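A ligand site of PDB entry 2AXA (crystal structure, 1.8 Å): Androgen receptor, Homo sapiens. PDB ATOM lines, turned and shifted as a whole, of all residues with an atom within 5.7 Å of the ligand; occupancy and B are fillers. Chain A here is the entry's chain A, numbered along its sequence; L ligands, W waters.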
ATOM      1  N   LEU A  38      -0.699  -5.459   2.894  1.00  0.00           N
ATOM      2  CA  LEU A  38       0.503  -4.615   2.902  1.00  0.00           C
ATOM      3  C   LEU A  38       1.460  -4.985   4.042  1.00  0.00           C
ATOM      4  O   LEU A  38       2.678  -4.932   3.886  1.00  0.00           O
ATOM      5  CB  LEU A  38       0.111  -3.136   2.960  1.00  0.00           C
ATOM      6  CG  LEU A  38       0.014  -2.407   1.608  1.00  0.00           C
ATOM      7  CD1 LEU A  38       1.406  -2.307   0.993  1.00  0.00           C
ATOM      8  CD2 LEU A  38      -0.938  -3.157   0.671  1.00  0.00           C
ATOM      9  N   LEU A  41       3.287  -7.762   2.732  1.00  0.00           N
ATOM     10  CA  LEU A  41       4.237  -7.379   1.691  1.00  0.00           C
ATOM     11  C   LEU A  41       5.474  -6.757   2.375  1.00  0.00           C
ATOM     12  O   LEU A  41       6.593  -7.006   1.956  1.00  0.00           O
ATOM     13  CB  LEU A  41       3.599  -6.378   0.710  1.00  0.00           C
ATOM     14  CG  LEU A  41       2.722  -6.996  -0.395  1.00  0.00           C
ATOM     15  CD1 LEU A  41       2.041  -5.905  -1.226  1.00  0.00           C
ATOM     16  CD2 LEU A  41       3.582  -7.875  -1.307  1.00  0.00           C
ATOM     17  N   ASN A  42       5.260  -5.985   3.439  1.00  0.00           N
ATOM     18  CA  ASN A  42       6.380  -5.365   4.163  1.00  0.00           C
ATOM     19  C   ASN A  42       7.244  -6.417   4.839  1.00  0.00           C
ATOM     20  O   ASN A  42       8.470  -6.374   4.745  1.00  0.00           O
ATOM     21  CB  ASN A  42       5.872  -4.374   5.214  1.00  0.00           C
ATOM     22  CG  ASN A  42       5.219  -3.149   4.617  1.00  0.00           C
ATOM     23  OD1 ASN A  42       5.356  -2.879   3.421  1.00  0.00           O
ATOM     24  ND2 ASN A  42       4.526  -2.384   5.445  1.00  0.00           N
ATOM     25  N   GLU A  43       6.604  -7.364   5.517  1.00  0.00           N
ATOM     26  CA  GLU A  43       7.311  -8.431   6.204  1.00  0.00           C
ATOM     27  C   GLU A  43       8.067  -9.262   5.174  1.00  0.00           C
ATOM     28  O   GLU A  43       9.237  -9.602   5.373  1.00  0.00           O
ATOM     29  CB  GLU A  43       6.323  -9.323   6.971  1.00  0.00           C
ATOM     30  CG  GLU A  43       6.938 -10.588   7.563  1.00  0.00           C
ATOM     31  CD  GLU A  43       7.966 -10.313   8.656  1.00  0.00           C
ATOM     32  OE1 GLU A  43       8.817 -11.187   8.905  1.00  0.00           O
ATOM     33  OE2 GLU A  43       7.911  -9.232   9.276  1.00  0.00           O
ATOM     34  N   LEU A  44       7.413  -9.593   4.062  1.00  0.00           N
ATOM     35  CA  LEU A  44       8.056 -10.369   3.003  1.00  0.00           C
ATOM     36  C   LEU A  44       9.264  -9.599   2.466  1.00  0.00           C
ATOM     37  O   LEU A  44      10.331 -10.174   2.262  1.00  0.00           O
ATOM     38  CB  LEU A  44       7.090 -10.667   1.863  1.00  0.00           C
ATOM     39  CG  LEU A  44       7.704 -11.420   0.670  1.00  0.00           C
ATOM     40  CD1 LEU A  44       8.278 -12.757   1.120  1.00  0.00           C
ATOM     41  CD2 LEU A  44       6.651 -11.638  -0.401  1.00  0.00           C
ATOM     42  N   GLY A  45       9.079  -8.298   2.247  1.00  0.00           N
ATOM     43  CA  GLY A  45      10.168  -7.479   1.733  1.00  0.00           C
ATOM     44  C   GLY A  45      11.386  -7.555   2.623  1.00  0.00           C
ATOM     45  O   GLY A  45      12.506  -7.713   2.151  1.00  0.00           O
ATOM     46  N   GLN A  48      13.082 -10.941   2.444  1.00  0.00           N
ATOM     47  CA  GLN A  48      13.839 -11.059   1.217  1.00  0.00           C
ATOM     48  C   GLN A  48      15.143 -10.239   1.279  1.00  0.00           C
ATOM     49  O   GLN A  48      16.159 -10.664   0.732  1.00  0.00           O
ATOM     50  CB  GLN A  48      12.998 -10.611   0.017  1.00  0.00           C
ATOM     51  CG  GLN A  48      11.775 -11.506  -0.207  1.00  0.00           C
ATOM     52  CD  GLN A  48      11.201 -11.387  -1.611  1.00  0.00           C
ATOM     53  OE1 GLN A  48      10.200 -12.029  -1.927  1.00  0.00           O
ATOM     54  NE2 GLN A  48      11.842 -10.585  -2.451  1.00  0.00           N
ATOM     55  N   GLN A  75      20.673  -1.340  -0.835  1.00  0.00           N
ATOM     56  CA  GLN A  75      19.455  -0.650  -0.426  1.00  0.00           C
ATOM     57  C   GLN A  75      18.731   0.033  -1.586  1.00  0.00           C
ATOM     58  O   GLN A  75      17.504  -0.025  -1.671  1.00  0.00           O
ATOM     59  CB  GLN A  75      19.774   0.339   0.704  1.00  0.00           C
ATOM     60  CG  GLN A  75      20.389  -0.340   1.923  1.00  0.00           C
ATOM     61  CD  GLN A  75      20.552   0.588   3.121  1.00  0.00           C
ATOM     62  OE1 GLN A  75      20.778   1.787   2.970  1.00  0.00           O
ATOM     63  NE2 GLN A  75      20.470   0.022   4.317  1.00  0.00           N
ATOM     64  N   TRP A  78      17.378  -2.790  -4.011  1.00  0.00           N
ATOM     65  CA  TRP A  78      16.474  -3.711  -3.329  1.00  0.00           C
ATOM     66  C   TRP A  78      15.133  -3.929  -4.030  1.00  0.00           C
ATOM     67  O   TRP A  78      14.784  -5.054  -4.375  1.00  0.00           O
ATOM     68  CB  TRP A  78      16.288  -3.227  -1.883  1.00  0.00           C
ATOM     69  CG  TRP A  78      15.403  -4.071  -1.020  1.00  0.00           C
ATOM     70  CD1 TRP A  78      15.031  -5.374  -1.220  1.00  0.00           C
ATOM     71  CD2 TRP A  78      14.792  -3.665   0.210  1.00  0.00           C
ATOM     72  NE1 TRP A  78      14.219  -5.796  -0.192  1.00  0.00           N
ATOM     73  CE2 TRP A  78      14.059  -4.768   0.706  1.00  0.00           C
ATOM     74  CE3 TRP A  78      14.798  -2.464   0.945  1.00  0.00           C
ATOM     75  CZ2 TRP A  78      13.336  -4.706   1.902  1.00  0.00           C
ATOM     76  CZ3 TRP A  78      14.079  -2.412   2.132  1.00  0.00           C
ATOM     77  CH2 TRP A  78      13.360  -3.524   2.599  1.00  0.00           C
ATOM     78  N   MET A  79      14.370  -2.854  -4.234  1.00  0.00           N
ATOM     79  CA  MET A  79      13.064  -2.972  -4.887  1.00  0.00           C
ATOM     80  C   MET A  79      13.172  -3.595  -6.285  1.00  0.00           C
ATOM     81  O   MET A  79      12.462  -4.547  -6.596  1.00  0.00           O
ATOM     82  CB  MET A  79      12.392  -1.596  -4.980  1.00  0.00           C
ATOM     83  CG  MET A  79      10.980  -1.640  -5.553  1.00  0.00           C
ATOM     84  SD  MET A  79       9.798  -2.429  -4.448  1.00  0.00           S
ATOM     85  CE  MET A  79       9.302  -1.024  -3.403  1.00  0.00           C
ATOM     86  N   MET A  82      13.893  -7.336  -6.324  1.00  0.00           N
ATOM     87  CA  MET A  82      12.731  -8.129  -5.945  1.00  0.00           C
ATOM     88  C   MET A  82      11.707  -8.198  -7.076  1.00  0.00           C
ATOM     89  O   MET A  82      11.122  -9.249  -7.322  1.00  0.00           O
ATOM     90  CB  MET A  82      12.067  -7.577  -4.684  1.00  0.00           C
ATOM     91  CG  MET A  82      12.874  -7.717  -3.396  1.00  0.00           C
ATOM     92  SD  MET A  82      11.815  -7.556  -1.914  1.00  0.00           S
ATOM     93  CE  MET A  82      11.394  -5.831  -1.981  1.00  0.00           C
ATOM     94  N   VAL A  83      11.486  -7.064  -7.747  1.00  0.00           N
ATOM     95  CA  VAL A  83      10.535  -6.996  -8.846  1.00  0.00           C
ATOM     96  C   VAL A  83      10.928  -7.980  -9.949  1.00  0.00           C
ATOM     97  O   VAL A  83      10.099  -8.735 -10.450  1.00  0.00           O
ATOM     98  CB  VAL A  83      10.473  -5.574  -9.474  1.00  0.00           C
ATOM     99  CG1 VAL A  83       9.776  -5.615 -10.828  1.00  0.00           C
ATOM    100  CG2 VAL A  83       9.714  -4.625  -8.541  1.00  0.00           C
ATOM    101  N   PHE A  84      12.202  -7.954 -10.324  1.00  0.00           N
ATOM    102  CA  PHE A  84      12.707  -8.815 -11.382  1.00  0.00           C
ATOM    103  C   PHE A  84      12.560 -10.293 -11.032  1.00  0.00           C
ATOM    104  O   PHE A  84      12.102 -11.079 -11.848  1.00  0.00           O
ATOM    105  CB  PHE A  84      14.175  -8.479 -11.666  1.00  0.00           C
ATOM    106  CG  PHE A  84      14.699  -9.063 -12.944  1.00  0.00           C
ATOM    107  CD1 PHE A  84      14.152  -8.686 -14.171  1.00  0.00           C
ATOM    108  CD2 PHE A  84      15.764  -9.952 -12.933  1.00  0.00           C
ATOM    109  CE1 PHE A  84      14.660  -9.200 -15.368  1.00  0.00           C
ATOM    110  CE2 PHE A  84      16.276 -10.475 -14.129  1.00  0.00           C
ATOM    111  CZ  PHE A  84      15.724 -10.088 -15.348  1.00  0.00           C
ATOM    112  N   ALA A  85      12.934 -10.648  -9.799  1.00  0.00           N
ATOM    113  CA  ALA A  85      12.839 -12.035  -9.369  1.00  0.00           C
ATOM    114  C   ALA A  85      11.373 -12.465  -9.204  1.00  0.00           C
ATOM    115  O   ALA A  85      11.043 -13.620  -9.433  1.00  0.00           O
ATOM    116  CB  ALA A  85      13.594 -12.227  -8.043  1.00  0.00           C
ATOM    117  N   MET A  86      10.501 -11.543  -8.813  1.00  0.00           N
ATOM    118  CA  MET A  86       9.096 -11.888  -8.639  1.00  0.00           C
ATOM    119  C   MET A  86       8.483 -12.191  -9.996  1.00  0.00           C
ATOM    120  O   MET A  86       7.690 -13.134 -10.139  1.00  0.00           O
ATOM    121  CB  MET A  86       8.349 -10.744  -7.934  1.00  0.00           C
ATOM    122  CG  MET A  86       6.951 -11.116  -7.423  1.00  0.00           C
ATOM    123  SD  MET A  86       5.696 -11.002  -8.712  1.00  0.00           S
ATOM    124  CE  MET A  86       5.282  -9.250  -8.612  1.00  0.00           C
ATOM    125  N   ARG A  89       9.466 -15.697 -11.024  1.00  0.00           N
ATOM    126  CA  ARG A  89       8.719 -16.715 -10.277  1.00  0.00           C
ATOM    127  C   ARG A  89       7.286 -16.804 -10.784  1.00  0.00           C
ATOM    128  O   ARG A  89       6.692 -17.885 -10.814  1.00  0.00           O
ATOM    129  CB  ARG A  89       8.664 -16.374  -8.780  1.00  0.00           C
ATOM    130  CG  ARG A  89       9.985 -16.524  -8.030  1.00  0.00           C
ATOM    131  CD  ARG A  89       9.733 -16.547  -6.515  1.00  0.00           C
ATOM    132  NE  ARG A  89       9.131 -15.310  -6.013  1.00  0.00           N
ATOM    133  CZ  ARG A  89       9.808 -14.194  -5.765  1.00  0.00           C
ATOM    134  NH1 ARG A  89      11.111 -14.143  -5.971  1.00  0.00           N
ATOM    135  NH2 ARG A  89       9.178 -13.120  -5.301  1.00  0.00           N
ATOM    136  N   TYR A 100       3.366 -14.154  -8.206  1.00  0.00           N
ATOM    137  CA  TYR A 100       3.887 -15.036  -7.182  1.00  0.00           C
ATOM    138  C   TYR A 100       4.896 -14.319  -6.271  1.00  0.00           C
ATOM    139  O   TYR A 100       6.097 -14.543  -6.380  1.00  0.00           O
ATOM    140  CB  TYR A 100       4.556 -16.224  -7.872  1.00  0.00           C
ATOM    141  CG  TYR A 100       4.657 -17.492  -7.063  1.00  0.00           C
ATOM    142  CD1 TYR A 100       3.674 -18.465  -7.122  1.00  0.00           C
ATOM    143  CD2 TYR A 100       5.790 -17.756  -6.289  1.00  0.00           C
ATOM    144  CE1 TYR A 100       3.811 -19.681  -6.451  1.00  0.00           C
ATOM    145  CE2 TYR A 100       5.945 -18.963  -5.609  1.00  0.00           C
ATOM    146  CZ  TYR A 100       4.953 -19.920  -5.690  1.00  0.00           C
ATOM    147  OH  TYR A 100       5.127 -21.124  -5.050  1.00  0.00           O
ATOM    148  N   PHE A 101       4.416 -13.458  -5.373  1.00  0.00           N
ATOM    149  CA  PHE A 101       5.325 -12.765  -4.469  1.00  0.00           C
ATOM    150  C   PHE A 101       6.008 -13.803  -3.585  1.00  0.00           C
ATOM    151  O   PHE A 101       7.185 -13.676  -3.237  1.00  0.00           O
ATOM    152  CB  PHE A 101       4.587 -11.768  -3.583  1.00  0.00           C
ATOM    153  CG  PHE A 101       4.061 -10.571  -4.316  1.00  0.00           C
ATOM    154  CD1 PHE A 101       2.815 -10.601  -4.930  1.00  0.00           C
ATOM    155  CD2 PHE A 101       4.808  -9.401  -4.377  1.00  0.00           C
ATOM    156  CE1 PHE A 101       2.303  -9.475  -5.583  1.00  0.00           C
ATOM    157  CE2 PHE A 101       4.313  -8.267  -5.031  1.00  0.00           C
ATOM    158  CZ  PHE A 101       3.063  -8.308  -5.633  1.00  0.00           C
ATOM    159  N   ALA A 102       5.257 -14.832  -3.210  1.00  0.00           N
ATOM    160  CA  ALA A 102       5.745 -15.932  -2.379  1.00  0.00           C
ATOM    161  C   ALA A 102       4.716 -17.052  -2.469  1.00  0.00           C
ATOM    162  O   ALA A 102       3.586 -16.828  -2.905  1.00  0.00           O
ATOM    163  CB  ALA A 102       5.898 -15.471  -0.927  1.00  0.00           C
ATOM    164  N   MET A 117      -2.145  -1.136  -5.389  1.00  0.00           N
ATOM    165  CA  MET A 117      -0.928  -1.130  -6.195  1.00  0.00           C
ATOM    166  C   MET A 117      -1.266  -1.800  -7.510  1.00  0.00           C
ATOM    167  O   MET A 117      -0.429  -2.469  -8.117  1.00  0.00           O
ATOM    168  CB  MET A 117       0.169  -1.967  -5.525  1.00  0.00           C
ATOM    169  CG  MET A 117       0.493  -1.598  -4.098  1.00  0.00           C
ATOM    170  SD  MET A 117       1.508  -2.878  -3.319  1.00  0.00           S
ATOM    171  CE  MET A 117       3.055  -2.521  -4.028  1.00  0.00           C
ATOM    172  N   MET A 124       4.039  -5.522 -13.592  1.00  0.00           N
ATOM    173  CA  MET A 124       4.887  -6.649 -13.238  1.00  0.00           C
ATOM    174  C   MET A 124       4.335  -7.918 -13.879  1.00  0.00           C
ATOM    175  O   MET A 124       5.094  -8.845 -14.179  1.00  0.00           O
ATOM    176  CB  MET A 124       4.969  -6.807 -11.712  1.00  0.00           C
ATOM    177  CG  MET A 124       5.607  -5.601 -11.012  1.00  0.00           C
ATOM    178  SD  MET A 124       6.022  -5.867  -9.276  1.00  0.00           S
ATOM    179  CE  MET A 124       4.397  -5.800  -8.534  1.00  0.00           C
ATOM    180  N   LEU A 210       6.660   1.727  -7.376  1.00  0.00           N
ATOM    181  CA  LEU A 210       6.505   1.039  -6.103  1.00  0.00           C
ATOM    182  C   LEU A 210       7.122   1.874  -4.979  1.00  0.00           C
ATOM    183  O   LEU A 210       6.571   1.955  -3.886  1.00  0.00           O
ATOM    184  CB  LEU A 210       7.165  -0.353  -6.160  1.00  0.00           C
ATOM    185  CG  LEU A 210       6.448  -1.376  -7.037  1.00  0.00           C
ATOM    186  CD1 LEU A 210       7.319  -2.592  -7.236  1.00  0.00           C
ATOM    187  CD2 LEU A 210       5.124  -1.773  -6.390  1.00  0.00           C
ATOM    188  N   HIS A 211       8.257   2.491  -5.264  1.00  0.00           N
ATOM    189  CA  HIS A 211       8.930   3.332  -4.281  1.00  0.00           C
ATOM    190  C   HIS A 211       8.045   4.502  -3.894  1.00  0.00           C
ATOM    191  O   HIS A 211       7.933   4.839  -2.710  1.00  0.00           O
ATOM    192  CB  HIS A 211      10.250   3.870  -4.856  1.00  0.00           C
ATOM    193  CG  HIS A 211      11.422   2.958  -4.650  1.00  0.00           C
ATOM    194  ND1 HIS A 211      12.505   2.941  -5.495  1.00  0.00           N
ATOM    195  CD2 HIS A 211      11.688   2.053  -3.676  1.00  0.00           C
ATOM    196  CE1 HIS A 211      13.398   2.068  -5.054  1.00  0.00           C
ATOM    197  NE2 HIS A 211      12.920   1.521  -3.945  1.00  0.00           N
ATOM    198  N   PHE A 213       4.741   4.731  -4.150  1.00  0.00           N
ATOM    199  CA  PHE A 213       3.598   4.207  -3.414  1.00  0.00           C
ATOM    200  C   PHE A 213       3.988   3.888  -1.974  1.00  0.00           C
ATOM    201  O   PHE A 213       3.315   4.302  -1.038  1.00  0.00           O
ATOM    202  CB  PHE A 213       3.061   2.947  -4.116  1.00  0.00           C
ATOM    203  CG  PHE A 213       2.167   2.099  -3.253  1.00  0.00           C
ATOM    204  CD1 PHE A 213       2.708   1.069  -2.481  1.00  0.00           C
ATOM    205  CD2 PHE A 213       0.797   2.327  -3.206  1.00  0.00           C
ATOM    206  CE1 PHE A 213       1.889   0.293  -1.667  1.00  0.00           C
ATOM    207  CE2 PHE A 213      -0.026   1.560  -2.394  1.00  0.00           C
ATOM    208  CZ  PHE A 213       0.524   0.534  -1.623  1.00  0.00           C
ATOM    209  N   THR A 214       5.093   3.148  -1.822  1.00  0.00           N
ATOM    210  CA  THR A 214       5.585   2.759  -0.503  1.00  0.00           C
ATOM    211  C   THR A 214       5.922   3.991   0.332  1.00  0.00           C
ATOM    212  O   THR A 214       5.680   4.007   1.539  1.00  0.00           O
ATOM    213  CB  THR A 214       6.844   1.884  -0.623  1.00  0.00           C
ATOM    214  OG1 THR A 214       6.550   0.732  -1.418  1.00  0.00           O
ATOM    215  CG2 THR A 214       7.320   1.441   0.754  1.00  0.00           C
ATOM    216  N   LEU A 217       2.715   5.590   1.476  1.00  0.00           N
ATOM    217  CA  LEU A 217       2.104   4.714   2.487  1.00  0.00           C
ATOM    218  C   LEU A 217       2.753   4.891   3.862  1.00  0.00           C
ATOM    219  O   LEU A 217       2.044   5.020   4.857  1.00  0.00           O
ATOM    220  CB  LEU A 217       2.186   3.248   2.031  1.00  0.00           C
ATOM    221  CG  LEU A 217       1.489   2.207   2.923  1.00  0.00           C
ATOM    222  CD1 LEU A 217       0.055   2.602   3.188  1.00  0.00           C
ATOM    223  CD2 LEU A 217       1.551   0.835   2.252  1.00  0.00           C
ATOM    224  N   PHE A 228       5.017  -1.238   9.421  1.00  0.00           N
ATOM    225  CA  PHE A 228       6.292  -1.178   8.730  1.00  0.00           C
ATOM    226  C   PHE A 228       7.428  -1.632   9.640  1.00  0.00           C
ATOM    227  O   PHE A 228       7.608  -1.099  10.730  1.00  0.00           O
ATOM    228  CB  PHE A 228       6.600   0.243   8.247  1.00  0.00           C
ATOM    229  CG  PHE A 228       5.940   0.592   6.951  1.00  0.00           C
ATOM    230  CD1 PHE A 228       4.699   1.211   6.925  1.00  0.00           C
ATOM    231  CD2 PHE A 228       6.555   0.279   5.738  1.00  0.00           C
ATOM    232  CE1 PHE A 228       4.072   1.521   5.716  1.00  0.00           C
ATOM    233  CE2 PHE A 228       5.941   0.585   4.530  1.00  0.00           C
ATOM    234  CZ  PHE A 228       4.700   1.205   4.514  1.00  0.00           C
ATOM    235  N   MET A 232      12.995  -1.494   7.194  1.00  0.00           N
ATOM    236  CA  MET A 232      12.345  -1.006   5.991  1.00  0.00           C
ATOM    237  C   MET A 232      11.973   0.463   6.141  1.00  0.00           C
ATOM    238  O   MET A 232      12.221   1.254   5.228  1.00  0.00           O
ATOM    239  CB  MET A 232      11.085  -1.830   5.677  1.00  0.00           C
ATOM    240  CG  MET A 232      10.367  -1.370   4.406  1.00  0.00           C
ATOM    241  SD  MET A 232       8.909  -2.378   3.974  1.00  0.00           S
ATOM    242  CE  MET A 232       9.727  -3.849   3.314  1.00  0.00           C
ATOM    243  N   ILE A 235      14.986   2.626   5.695  1.00  0.00           N
ATOM    244  CA  ILE A 235      15.400   2.693   4.287  1.00  0.00           C
ATOM    245  C   ILE A 235      14.469   3.558   3.443  1.00  0.00           C
ATOM    246  O   ILE A 235      14.925   4.333   2.606  1.00  0.00           O
ATOM    247  CB  ILE A 235      15.468   1.267   3.684  1.00  0.00           C
ATOM    248  CG1 ILE A 235      16.696   0.542   4.259  1.00  0.00           C
ATOM    249  CG2 ILE A 235      15.544   1.342   2.161  1.00  0.00           C
ATOM    250  CD1 ILE A 235      16.827  -0.908   3.832  1.00  0.00           C
ATOM    251  N   ILE A 236      13.162   3.443   3.678  1.00  0.00           N
ATOM    252  CA  ILE A 236      12.185   4.225   2.936  1.00  0.00           C
ATOM    253  C   ILE A 236      12.317   5.710   3.240  1.00  0.00           C
ATOM    254  O   ILE A 236      12.109   6.545   2.368  1.00  0.00           O
ATOM    255  CB  ILE A 236      10.725   3.802   3.292  1.00  0.00           C
ATOM    256  CG1 ILE A 236      10.505   2.337   2.944  1.00  0.00           C
ATOM    257  CG2 ILE A 236       9.725   4.681   2.527  1.00  0.00           C
ATOM    258  CD1 ILE A 236       9.186   1.788   3.440  1.00  0.00           C
ATOM    259  N   VAL A 240      15.157   5.827  -0.027  1.00  0.00           N
ATOM    260  CA  VAL A 240      14.159   6.003  -1.081  1.00  0.00           C
ATOM    261  C   VAL A 240      13.926   7.463  -1.514  1.00  0.00           C
ATOM    262  O   VAL A 240      13.732   7.739  -2.704  1.00  0.00           O
ATOM    263  CB  VAL A 240      12.832   5.340  -0.660  1.00  0.00           C
ATOM    264  CG1 VAL A 240      11.716   5.693  -1.638  1.00  0.00           C
ATOM    265  CG2 VAL A 240      13.020   3.816  -0.613  1.00  0.00           C
HETATM  266  C1  LIG L   1      10.183  -0.664   0.493  1.00  0.00           C
HETATM  267  C2  LIG L   1      11.311   0.091   0.190  1.00  0.00           C
HETATM  268  C3  LIG L   1      12.331  -0.442  -0.586  1.00  0.00           C
HETATM  269  F1  LIG L   1      13.443   0.278  -0.854  1.00  0.00           F
HETATM  270  C4  LIG L   1      12.222  -1.754  -1.064  1.00  0.00           C
HETATM  271  C5  LIG L   1      11.094  -2.507  -0.751  1.00  0.00           C
HETATM  272  C6  LIG L   1      10.074  -1.975   0.024  1.00  0.00           C
HETATM  273  O1  LIG L   1       8.987  -2.751   0.281  1.00  0.00           O
HETATM  274  C7  LIG L   1       7.731  -2.052   0.244  1.00  0.00           C
HETATM  275  C8  LIG L   1       6.620  -3.089   0.142  1.00  0.00           C
HETATM  276  O2  LIG L   1       6.619  -3.885   1.330  1.00  0.00           O
HETATM  277  C9  LIG L   1       5.274  -2.371  -0.020  1.00  0.00           C
HETATM  278  C10 LIG L   1       6.880  -3.982  -1.067  1.00  0.00           C
HETATM  279  O3  LIG L   1       6.868  -3.517  -2.210  1.00  0.00           O
HETATM  280  N1  LIG L   1       7.133  -5.253  -0.770  1.00  0.00           N
HETATM  281  C11 LIG L   1       7.392  -6.231  -1.634  1.00  0.00           C
HETATM  282  C12 LIG L   1       7.512  -6.015  -3.004  1.00  0.00           C
HETATM  283  C13 LIG L   1       7.637  -7.511  -1.134  1.00  0.00           C
HETATM  284  C14 LIG L   1       8.003  -8.529  -2.001  1.00  0.00           C
HETATM  285  C15 LIG L   1       8.131  -8.310  -3.372  1.00  0.00           C
HETATM  286  N2  LIG L   1       8.525  -9.352  -4.105  1.00  0.00           N
HETATM  287  O4  LIG L   1       8.909  -9.237  -5.469  1.00  0.00           O
HETATM  288  O5  LIG L   1       8.724 -10.612  -3.477  1.00  0.00           O
HETATM  289  C16 LIG L   1       7.869  -7.041  -3.891  1.00  0.00           C
HETATM  290  C17 LIG L   1       7.910  -6.714  -5.398  1.00  0.00           C
HETATM  291  F2  LIG L   1       9.174  -6.597  -5.805  1.00  0.00           F
HETATM  292  F3  LIG L   1       7.297  -7.637  -6.136  1.00  0.00           F
HETATM  293  F4  LIG L   1       7.299  -5.571  -5.691  1.00  0.00           F
HETATM  294  O   HOH W   1      15.229  -0.129  -3.355  1.00  0.00           O
HETATM  295  O   HOH W   2      11.556 -11.125  -5.297  1.00  0.00           O
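The side-chain amide oxygen of Gln 48 lies close to an oxygen (O5) of the ligand, 2.6 Å away.
N of Asn 42 lies close to O2 of the ligand (3.3 Å).
OD1 of Asn 42 sits at hydrogen-bond distance from O2 of the ligand.
An oxygen (O5) of the ligand is in hydrogen-bond range of the guanidinium group (NH2) of Arg 89, 3.1 Å away.
O2 of the ligand is in hydrogen-bond range of O of Leu 41 (3.2 Å).
Water W1 lies within hydrogen-bond range of O of Gln 75, NE2 of His 211, N of Met 79 and N of Trp 78.
Water W2 lies within hydrogen-bond range of O of Met 82 (2.8 Å), NE2 of Gln 48 (2.9 Å), NH2 of Arg 89 (3.1 Å) and O4 of the ligand (3.3 Å).
O4 of the ligand lies close to O of Met 82 (2.9 Å).
N of Val 83 lies close to F2 of the ligand (3.1 Å).
The backbone carbonyl oxygen of Phe 101 lies close to an oxygen (O5) of the ligand.
A ring nitrogen (NE2) of His 211 sits close to a fluorine (F1) of the ligand (3.4 Å).
O1 of the ligand lies close to SD of Met 232.
CD1 of Leu 38 touches C9 of the ligand, 3.999 Å away.
Leu 44 touches the ligand (CD2 to C14, 3.7 Å).
Gly 45 touches the ligand.
Trp 78 touches the ligand.
Met 79 touches the ligand (CE to C5, 3.5 Å).
Met 86 touches the ligand (CB to O4, 2.9 Å).
SD of Met 124 touches F4 of the ligand, at 3.8 Å.
CD1 of Leu 210 touches F4 of the ligand, at 3.4 Å.
Thr 214 touches the ligand.
Ile 235 touches the ligand (CG2 to F1, 3.8 Å).
CG1 of Ile 236 touches C2 of the ligand (3.6 Å).
Val 240 touches the ligand (CG2 to F1, 3.6 Å).
Hydrophobic or aromatic side chains within 4 Å of the ligand: Leu 38, Leu 41, Leu 44, Trp 78, Met 79, Met 82, Val 83, Met 86, Phe 101, Met 124, Leu 210, His 211, Met 232, Ile 235, Ile 236 and Val 240.
21 residues have an atom within 4 Å of the ligand: Leu 38, Leu 41, Asn 42, Leu 44, Gly 45, Gln 48, Trp 78, Met 79, Met 82, Val 83, Met 86, Arg 89, Phe 101, Met 124, Leu 210, His 211, Thr 214, Met 232, Ile 235, Ile 236 and Val 240.
Along chain A the residues within 4 Å of the ligand span positions 38 to 240.
NE2 of Gln 48 sits at hydrogen-bond distance from SD of Met 82, at 3.1 Å.
OD1 of Asn 42 sits close to SD of Met 232, at 3.6 Å.
O of Leu 38 lies close to OD1 of Asn 42, at 3.4 Å.
The side-chain sulfur (SD) of Met 82 sits close to the indole nitrogen (NE1) of Trp 78 (3.4 Å).
NH2 of Arg 89 lies within hydrogen-bond range of O of Phe 101, at 2.9 Å.
NE of Arg 89 is in hydrogen-bond range of O of Tyr 100 (3.2 Å).
The backbone carbonyl oxygen of Gly 45 lies close to the indole nitrogen of Trp 78, 3.5 Å away.
O of Leu 210 lies within hydrogen-bond range of OG1 of Thr 214 (2.8 Å).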
